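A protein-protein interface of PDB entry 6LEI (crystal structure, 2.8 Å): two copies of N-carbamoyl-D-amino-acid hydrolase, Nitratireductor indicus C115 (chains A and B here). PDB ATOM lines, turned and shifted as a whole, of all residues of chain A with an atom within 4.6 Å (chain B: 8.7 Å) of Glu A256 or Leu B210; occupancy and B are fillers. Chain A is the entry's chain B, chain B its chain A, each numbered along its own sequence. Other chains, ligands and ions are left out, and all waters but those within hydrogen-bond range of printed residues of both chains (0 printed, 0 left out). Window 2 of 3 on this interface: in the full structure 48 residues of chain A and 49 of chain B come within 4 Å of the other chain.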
ATOM      1  N   ILE A 250      26.957  15.549 -34.399  1.00  0.00           N
ATOM      2  CA  ILE A 250      26.099  16.680 -34.740  1.00  0.00           C
ATOM      3  C   ILE A 250      25.773  17.388 -33.431  1.00  0.00           C
ATOM      4  O   ILE A 250      25.198  16.779 -32.520  1.00  0.00           O
ATOM      5  CB  ILE A 250      24.816  16.239 -35.461  1.00  0.00           C
ATOM      6  CG1 ILE A 250      25.145  15.603 -36.813  1.00  0.00           C
ATOM      7  CG2 ILE A 250      23.871  17.419 -35.637  1.00  0.00           C
ATOM      8  CD1 ILE A 250      23.928  15.107 -37.565  1.00  0.00           C
ATOM      9  N   VAL A 251      26.143  18.662 -33.330  1.00  0.00           N
ATOM     10  CA  VAL A 251      26.062  19.409 -32.079  1.00  0.00           C
ATOM     11  C   VAL A 251      24.946  20.439 -32.172  1.00  0.00           C
ATOM     12  O   VAL A 251      24.801  21.126 -33.190  1.00  0.00           O
ATOM     13  CB  VAL A 251      27.404  20.086 -31.741  1.00  0.00           C
ATOM     14  CG1 VAL A 251      27.414  20.548 -30.293  1.00  0.00           C
ATOM     15  CG2 VAL A 251      28.561  19.136 -32.012  1.00  0.00           C
ATOM     16  N   ALA A 252      24.169  20.552 -31.099  1.00  0.00           N
ATOM     17  CA  ALA A 252      23.043  21.472 -31.026  1.00  0.00           C
ATOM     18  C   ALA A 252      23.520  22.860 -30.606  1.00  0.00           C
ATOM     19  O   ALA A 252      24.650  23.029 -30.143  1.00  0.00           O
ATOM     20  CB  ALA A 252      22.004  20.923 -30.051  1.00  0.00           C
ATOM     21  N   THR A 254      22.837  24.369 -28.032  1.00  0.00           N
ATOM     22  CA  THR A 254      23.124  24.318 -26.605  1.00  0.00           C
ATOM     23  C   THR A 254      24.445  23.624 -26.299  1.00  0.00           C
ATOM     24  O   THR A 254      24.758  23.407 -25.124  1.00  0.00           O
ATOM     25  CB  THR A 254      21.988  23.609 -25.863  1.00  0.00           C
ATOM     26  OG1 THR A 254      21.830  22.283 -26.382  1.00  0.00           O
ATOM     27  CG2 THR A 254      20.683  24.374 -26.028  1.00  0.00           C
ATOM     28  N   GLY A 255      25.220  23.276 -27.325  1.00  0.00           N
ATOM     29  CA  GLY A 255      26.424  22.497 -27.147  1.00  0.00           C
ATOM     30  C   GLY A 255      26.195  21.020 -26.920  1.00  0.00           C
ATOM     31  O   GLY A 255      27.174  20.273 -26.789  1.00  0.00           O
ATOM     32  N   GLU A 256      24.943  20.572 -26.873  1.00  0.00           N
ATOM     33  CA  GLU A 256      24.653  19.170 -26.611  1.00  0.00           C
ATOM     34  C   GLU A 256      24.931  18.314 -27.839  1.00  0.00           C
ATOM     35  O   GLU A 256      24.730  18.744 -28.979  1.00  0.00           O
ATOM     36  CB  GLU A 256      23.196  19.000 -26.186  1.00  0.00           C
ATOM     37  CG  GLU A 256      22.889  19.473 -24.778  1.00  0.00           C
ATOM     38  CD  GLU A 256      21.414  19.371 -24.452  1.00  0.00           C
ATOM     39  OE1 GLU A 256      20.601  19.947 -25.204  1.00  0.00           O
ATOM     40  OE2 GLU A 256      21.067  18.704 -23.454  1.00  0.00           O
ATOM     41  N   ILE A 257      25.393  17.092 -27.599  1.00  0.00           N
ATOM     42  CA  ILE A 257      25.601  16.110 -28.655  1.00  0.00           C
ATOM     43  C   ILE A 257      24.288  15.375 -28.882  1.00  0.00           C
ATOM     44  O   ILE A 257      23.790  14.681 -27.987  1.00  0.00           O
ATOM     45  CB  ILE A 257      26.727  15.131 -28.289  1.00  0.00           C
ATOM     46  CG1 ILE A 257      28.085  15.835 -28.341  1.00  0.00           C
ATOM     47  CG2 ILE A 257      26.692  13.909 -29.197  1.00  0.00           C
ATOM     48  CD1 ILE A 257      29.259  14.927 -28.042  1.00  0.00           C
ATOM     49  N   VAL A 258      23.717  15.533 -30.079  1.00  0.00           N
ATOM     50  CA  VAL A 258      22.442  14.898 -30.409  1.00  0.00           C
ATOM     51  C   VAL A 258      22.604  13.686 -31.317  1.00  0.00           C
ATOM     52  O   VAL A 258      21.638  12.924 -31.488  1.00  0.00           O
ATOM     53  CB  VAL A 258      21.464  15.906 -31.052  1.00  0.00           C
ATOM     54  CG1 VAL A 258      21.198  17.068 -30.106  1.00  0.00           C
ATOM     55  CG2 VAL A 258      22.007  16.403 -32.384  1.00  0.00           C
ATOM     56  N   ARG A 277      16.089  26.903 -32.982  1.00  0.00           N
ATOM     57  CA  ARG A 277      16.696  26.801 -31.661  1.00  0.00           C
ATOM     58  C   ARG A 277      17.934  27.677 -31.518  1.00  0.00           C
ATOM     59  O   ARG A 277      18.420  27.855 -30.396  1.00  0.00           O
ATOM     60  CB  ARG A 277      17.056  25.346 -31.354  1.00  0.00           C
ATOM     61  CG  ARG A 277      15.854  24.431 -31.168  1.00  0.00           C
ATOM     62  CD  ARG A 277      16.289  22.990 -30.932  1.00  0.00           C
ATOM     63  NE  ARG A 277      17.160  22.861 -29.766  1.00  0.00           N
ATOM     64  CZ  ARG A 277      17.744  21.728 -29.392  1.00  0.00           C
ATOM     65  NH1 ARG A 277      17.554  20.618 -30.093  1.00  0.00           N
ATOM     66  NH2 ARG A 277      18.522  21.702 -28.318  1.00  0.00           N
ATOM     67  N   TYR A 281      19.410  32.035 -27.819  1.00  0.00           N
ATOM     68  CA  TYR A 281      20.669  32.527 -27.266  1.00  0.00           C
ATOM     69  C   TYR A 281      21.135  33.798 -27.965  1.00  0.00           C
ATOM     70  O   TYR A 281      21.765  34.654 -27.334  1.00  0.00           O
ATOM     71  CB  TYR A 281      21.749  31.450 -27.360  1.00  0.00           C
ATOM     72  CG  TYR A 281      21.542  30.268 -26.438  1.00  0.00           C
ATOM     73  CD1 TYR A 281      20.764  30.380 -25.293  1.00  0.00           C
ATOM     74  CD2 TYR A 281      22.133  29.041 -26.712  1.00  0.00           C
ATOM     75  CE1 TYR A 281      20.578  29.301 -24.448  1.00  0.00           C
ATOM     76  CE2 TYR A 281      21.951  27.957 -25.873  1.00  0.00           C
ATOM     77  CZ  TYR A 281      21.173  28.093 -24.743  1.00  0.00           C
ATOM     78  OH  TYR A 281      20.991  27.015 -23.907  1.00  0.00           O
ATOM     79  N   ARG B 175      31.899  33.176 -20.546  1.00  0.00           N
ATOM     80  CA  ARG B 175      31.071  32.705 -21.648  1.00  0.00           C
ATOM     81  C   ARG B 175      31.596  33.142 -23.008  1.00  0.00           C
ATOM     82  O   ARG B 175      31.247  32.521 -24.019  1.00  0.00           O
ATOM     83  CB  ARG B 175      29.631  33.201 -21.482  1.00  0.00           C
ATOM     84  CG  ARG B 175      28.622  32.106 -21.173  1.00  0.00           C
ATOM     85  CD  ARG B 175      28.200  32.132 -19.714  1.00  0.00           C
ATOM     86  NE  ARG B 175      27.298  31.030 -19.388  1.00  0.00           N
ATOM     87  CZ  ARG B 175      26.713  30.868 -18.206  1.00  0.00           C
ATOM     88  NH1 ARG B 175      26.928  31.743 -17.233  1.00  0.00           N
ATOM     89  NH2 ARG B 175      25.908  29.835 -17.997  1.00  0.00           N
ATOM     90  N   VAL B 199      20.435  29.956 -10.766  1.00  0.00           N
ATOM     91  CA  VAL B 199      20.054  28.622 -11.222  1.00  0.00           C
ATOM     92  C   VAL B 199      19.007  28.710 -12.326  1.00  0.00           C
ATOM     93  O   VAL B 199      19.073  27.978 -13.322  1.00  0.00           O
ATOM     94  CB  VAL B 199      19.567  27.779 -10.029  1.00  0.00           C
ATOM     95  CG1 VAL B 199      18.727  26.606 -10.503  1.00  0.00           C
ATOM     96  CG2 VAL B 199      20.754  27.290  -9.216  1.00  0.00           C
ATOM     97  N   ASP B 201      16.780  30.577 -15.420  1.00  0.00           N
ATOM     98  CA  ASP B 201      17.018  31.477 -16.537  1.00  0.00           C
ATOM     99  C   ASP B 201      16.190  32.751 -16.363  1.00  0.00           C
ATOM    100  O   ASP B 201      15.486  32.935 -15.366  1.00  0.00           O
ATOM    101  CB  ASP B 201      16.700  30.774 -17.856  1.00  0.00           C
ATOM    102  CG  ASP B 201      17.377  31.427 -19.047  1.00  0.00           C
ATOM    103  OD1 ASP B 201      18.159  32.381 -18.841  1.00  0.00           O
ATOM    104  OD2 ASP B 201      17.125  30.991 -20.190  1.00  0.00           O
ATOM    105  N   GLU B 206      14.789  26.876 -15.292  1.00  0.00           N
ATOM    106  CA  GLU B 206      15.936  26.397 -14.530  1.00  0.00           C
ATOM    107  C   GLU B 206      16.986  25.756 -15.430  1.00  0.00           C
ATOM    108  O   GLU B 206      17.996  26.380 -15.758  1.00  0.00           O
ATOM    109  CB  GLU B 206      15.491  25.395 -13.460  1.00  0.00           C
ATOM    110  CG  GLU B 206      15.192  26.007 -12.099  1.00  0.00           C
ATOM    111  CD  GLU B 206      13.979  26.920 -12.111  1.00  0.00           C
ATOM    112  OE1 GLU B 206      13.876  27.779 -11.211  1.00  0.00           O
ATOM    113  OE2 GLU B 206      13.129  26.777 -13.014  1.00  0.00           O
ATOM    114  N   SER B 207      16.734  24.505 -15.824  1.00  0.00           N
ATOM    115  CA  SER B 207      17.688  23.696 -16.581  1.00  0.00           C
ATOM    116  C   SER B 207      19.021  23.606 -15.835  1.00  0.00           C
ATOM    117  O   SER B 207      20.068  24.054 -16.309  1.00  0.00           O
ATOM    118  CB  SER B 207      17.878  24.247 -17.999  1.00  0.00           C
ATOM    119  OG  SER B 207      16.645  24.305 -18.695  1.00  0.00           O
ATOM    120  N   GLU B 208      18.957  23.012 -14.640  1.00  0.00           N
ATOM    121  CA  GLU B 208      20.121  22.967 -13.757  1.00  0.00           C
ATOM    122  C   GLU B 208      21.278  22.211 -14.398  1.00  0.00           C
ATOM    123  O   GLU B 208      22.409  22.710 -14.445  1.00  0.00           O
ATOM    124  CB  GLU B 208      19.745  22.322 -12.424  1.00  0.00           C
ATOM    125  CG  GLU B 208      19.789  23.268 -11.239  1.00  0.00           C
ATOM    126  CD  GLU B 208      20.190  22.568  -9.956  1.00  0.00           C
ATOM    127  OE1 GLU B 208      21.405  22.475  -9.685  1.00  0.00           O
ATOM    128  OE2 GLU B 208      19.291  22.103  -9.225  1.00  0.00           O
ATOM    129  N   THR B 209      21.015  20.998 -14.886  1.00  0.00           N
ATOM    130  CA  THR B 209      22.084  20.188 -15.460  1.00  0.00           C
ATOM    131  C   THR B 209      22.657  20.834 -16.715  1.00  0.00           C
ATOM    132  O   THR B 209      23.862  20.738 -16.975  1.00  0.00           O
ATOM    133  CB  THR B 209      21.573  18.780 -15.764  1.00  0.00           C
ATOM    134  OG1 THR B 209      20.425  18.859 -16.620  1.00  0.00           O
ATOM    135  CG2 THR B 209      21.194  18.065 -14.477  1.00  0.00           C
ATOM    136  N   LEU B 210      21.811  21.499 -17.504  1.00  0.00           N
ATOM    137  CA  LEU B 210      22.296  22.172 -18.703  1.00  0.00           C
ATOM    138  C   LEU B 210      23.033  23.463 -18.372  1.00  0.00           C
ATOM    139  O   LEU B 210      23.961  23.844 -19.096  1.00  0.00           O
ATOM    140  CB  LEU B 210      21.133  22.458 -19.655  1.00  0.00           C
ATOM    141  CG  LEU B 210      21.523  22.904 -21.065  1.00  0.00           C
ATOM    142  CD1 LEU B 210      22.297  21.804 -21.777  1.00  0.00           C
ATOM    143  CD2 LEU B 210      20.295  23.307 -21.865  1.00  0.00           C
ATOM    144  N   ARG B 211      22.645  24.145 -17.293  1.00  0.00           N
ATOM    145  CA  ARG B 211      23.352  25.359 -16.897  1.00  0.00           C
ATOM    146  C   ARG B 211      24.711  25.034 -16.289  1.00  0.00           C
ATOM    147  O   ARG B 211      25.699  25.728 -16.555  1.00  0.00           O
ATOM    148  CB  ARG B 211      22.503  26.171 -15.922  1.00  0.00           C
ATOM    149  CG  ARG B 211      21.421  26.999 -16.590  1.00  0.00           C
ATOM    150  CD  ARG B 211      21.150  28.270 -15.805  1.00  0.00           C
ATOM    151  NE  ARG B 211      20.754  29.370 -16.679  1.00  0.00           N
ATOM    152  CZ  ARG B 211      20.742  30.647 -16.312  1.00  0.00           C
ATOM    153  NH1 ARG B 211      21.109  30.988 -15.085  1.00  0.00           N
ATOM    154  NH2 ARG B 211      20.369  31.583 -17.173  1.00  0.00           N
ATOM    155  N   MET B 212      24.780  23.985 -15.463  1.00  0.00           N
ATOM    156  CA  MET B 212      26.073  23.521 -14.972  1.00  0.00           C
ATOM    157  C   MET B 212      26.937  22.999 -16.112  1.00  0.00           C
ATOM    158  O   MET B 212      28.166  23.134 -16.076  1.00  0.00           O
ATOM    159  CB  MET B 212      25.875  22.438 -13.911  1.00  0.00           C
ATOM    160  CG  MET B 212      27.166  21.909 -13.305  1.00  0.00           C
ATOM    161  SD  MET B 212      28.045  23.147 -12.332  1.00  0.00           S
ATOM    162  CE  MET B 212      26.867  23.441 -11.017  1.00  0.00           C
ATOM    163  N   PHE B 213      26.312  22.402 -17.130  1.00  0.00           N
ATOM    164  CA  PHE B 213      27.048  21.965 -18.311  1.00  0.00           C
ATOM    165  C   PHE B 213      27.685  23.150 -19.027  1.00  0.00           C
ATOM    166  O   PHE B 213      28.868  23.113 -19.383  1.00  0.00           O
ATOM    167  CB  PHE B 213      26.110  21.198 -19.247  1.00  0.00           C
ATOM    168  CG  PHE B 213      26.678  20.952 -20.615  1.00  0.00           C
ATOM    169  CD1 PHE B 213      27.586  19.930 -20.831  1.00  0.00           C
ATOM    170  CD2 PHE B 213      26.287  21.733 -21.692  1.00  0.00           C
ATOM    171  CE1 PHE B 213      28.106  19.700 -22.092  1.00  0.00           C
ATOM    172  CE2 PHE B 213      26.802  21.507 -22.955  1.00  0.00           C
ATOM    173  CZ  PHE B 213      27.711  20.490 -23.155  1.00  0.00           C
ATOM    174  N   HIS B 214      26.911  24.217 -19.244  1.00  0.00           N
ATOM    175  CA  HIS B 214      27.462  25.413 -19.872  1.00  0.00           C
ATOM    176  C   HIS B 214      28.495  26.089 -18.980  1.00  0.00           C
ATOM    177  O   HIS B 214      29.442  26.703 -19.486  1.00  0.00           O
ATOM    178  CB  HIS B 214      26.343  26.393 -20.217  1.00  0.00           C
ATOM    179  CG  HIS B 214      25.390  25.881 -21.253  1.00  0.00           C
ATOM    180  ND1 HIS B 214      24.079  26.298 -21.329  1.00  0.00           N
ATOM    181  CD2 HIS B 214      25.561  24.991 -22.258  1.00  0.00           C
ATOM    182  CE1 HIS B 214      23.482  25.683 -22.335  1.00  0.00           C
ATOM    183  NE2 HIS B 214      24.359  24.885 -22.915  1.00  0.00           N
ATOM    184  N   ASN B 215      28.331  25.986 -17.658  1.00  0.00           N
ATOM    185  CA  ASN B 215      29.289  26.592 -16.740  1.00  0.00           C
ATOM    186  C   ASN B 215      30.677  25.989 -16.912  1.00  0.00           C
ATOM    187  O   ASN B 215      31.678  26.714 -16.943  1.00  0.00           O
ATOM    188  CB  ASN B 215      28.807  26.426 -15.298  1.00  0.00           C
ATOM    189  CG  ASN B 215      29.758  27.040 -14.287  1.00  0.00           C
ATOM    190  OD1 ASN B 215      30.416  28.043 -14.565  1.00  0.00           O
ATOM    191  ND2 ASN B 215      29.836  26.436 -13.108  1.00  0.00           N
ATOM    192  N   HIS B 216      30.758  24.662 -17.032  1.00  0.00           N
ATOM    193  CA  HIS B 216      32.053  24.007 -17.169  1.00  0.00           C
ATOM    194  C   HIS B 216      32.541  23.980 -18.613  1.00  0.00           C
ATOM    195  O   HIS B 216      33.748  24.091 -18.852  1.00  0.00           O
ATOM    196  CB  HIS B 216      31.981  22.584 -16.616  1.00  0.00           C
ATOM    197  CG  HIS B 216      31.805  22.522 -15.131  1.00  0.00           C
ATOM    198  ND1 HIS B 216      31.371  21.388 -14.480  1.00  0.00           N
ATOM    199  CD2 HIS B 216      32.010  23.452 -14.169  1.00  0.00           C
ATOM    200  CE1 HIS B 216      31.312  21.623 -13.180  1.00  0.00           C
ATOM    201  NE2 HIS B 216      31.696  22.869 -12.966  1.00  0.00           N
ATOM    202  N   LEU B 217      31.627  23.837 -19.578  1.00  0.00           N
ATOM    203  CA  LEU B 217      32.023  23.772 -20.983  1.00  0.00           C
ATOM    204  C   LEU B 217      32.803  25.011 -21.403  1.00  0.00           C
ATOM    205  O   LEU B 217      33.825  24.907 -22.092  1.00  0.00           O
ATOM    206  CB  LEU B 217      30.788  23.600 -21.868  1.00  0.00           C
ATOM    207  CG  LEU B 217      31.009  23.675 -23.380  1.00  0.00           C
ATOM    208  CD1 LEU B 217      31.759  22.448 -23.875  1.00  0.00           C
ATOM    209  CD2 LEU B 217      29.688  23.835 -24.116  1.00  0.00           C
ATOM    210  N   MET B 245      23.932  29.143  -8.401  1.00  0.00           N
ATOM    211  CA  MET B 245      24.585  27.896  -8.775  1.00  0.00           C
ATOM    212  C   MET B 245      25.975  27.799  -8.154  1.00  0.00           C
ATOM    213  O   MET B 245      26.709  28.787  -8.073  1.00  0.00           O
ATOM    214  CB  MET B 245      24.676  27.802 -10.298  1.00  0.00           C
ATOM    215  CG  MET B 245      25.815  26.949 -10.825  1.00  0.00           C
ATOM    216  SD  MET B 245      26.244  27.392 -12.518  1.00  0.00           S
ATOM    217  CE  MET B 245      24.655  27.222 -13.314  1.00  0.00           C
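NE2 of His B214 lies within hydrogen-bond range of O of Thr A254, 2.7 Å away.
OG1 of Thr A254 lies within hydrogen-bond range of OE1 of Glu A256 (2.9 Å). A ring nitrogen (ND1) of His B214 lies close to the backbone carbonyl oxygen of Leu B210 (3.3 Å).
Phe B213 touches Thr A254 (CE2 to O, 3.5 Å). CZ of Phe B213 touches O of Gly A255, 3.7 Å away. CD of Glu A256 touches CD1 of Leu B210, at 3.7 Å. OH of Tyr A281 touches CE1 of His B214, at 3.2 Å.
Of chain B, only Leu B210 (3.7 Å) comes within 4 Å of Glu A256. Leu B210 touches one residue of chain A. Ala A252 touches none of the printed residues of chain B. Printed residues of chain B within 4 Å of Thr A254: Phe B213 and His B214. Printed residues of chain A within 4 Å of Phe B213: Thr A254 (3.5 Å) and Gly A255 (3.7 Å). Of the printed residues of chain B, Tyr A281 touches His B214 (3.2 Å). The nearest residue of chain B that does not touch Glu A256 is Phe B213 (4.4 Å). The nearest printed residue of chain A that does not touch Leu B210 is Tyr A281 (4.3 Å).
Printed residues of chain A that touch a printed residue of chain B: Thr A254, Gly A255, Glu A256 and Tyr A281. Hydrophobic or aromatic side chains of chain A that line the printed part of chain B: Tyr A281. Along chain A the printed residues that touch a printed residue of chain B span positions 254 to 281. Of the 16 printed residues of chain B, 3 touch a printed residue of chain A. Among the printed residues, 5 pairs touch across the chains. Among the printed residues, no Asp or Glu carboxylate lies within 4 Å of a Lys or Arg side-chain nitrogen of the other chain.
No position is printed for both chains.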
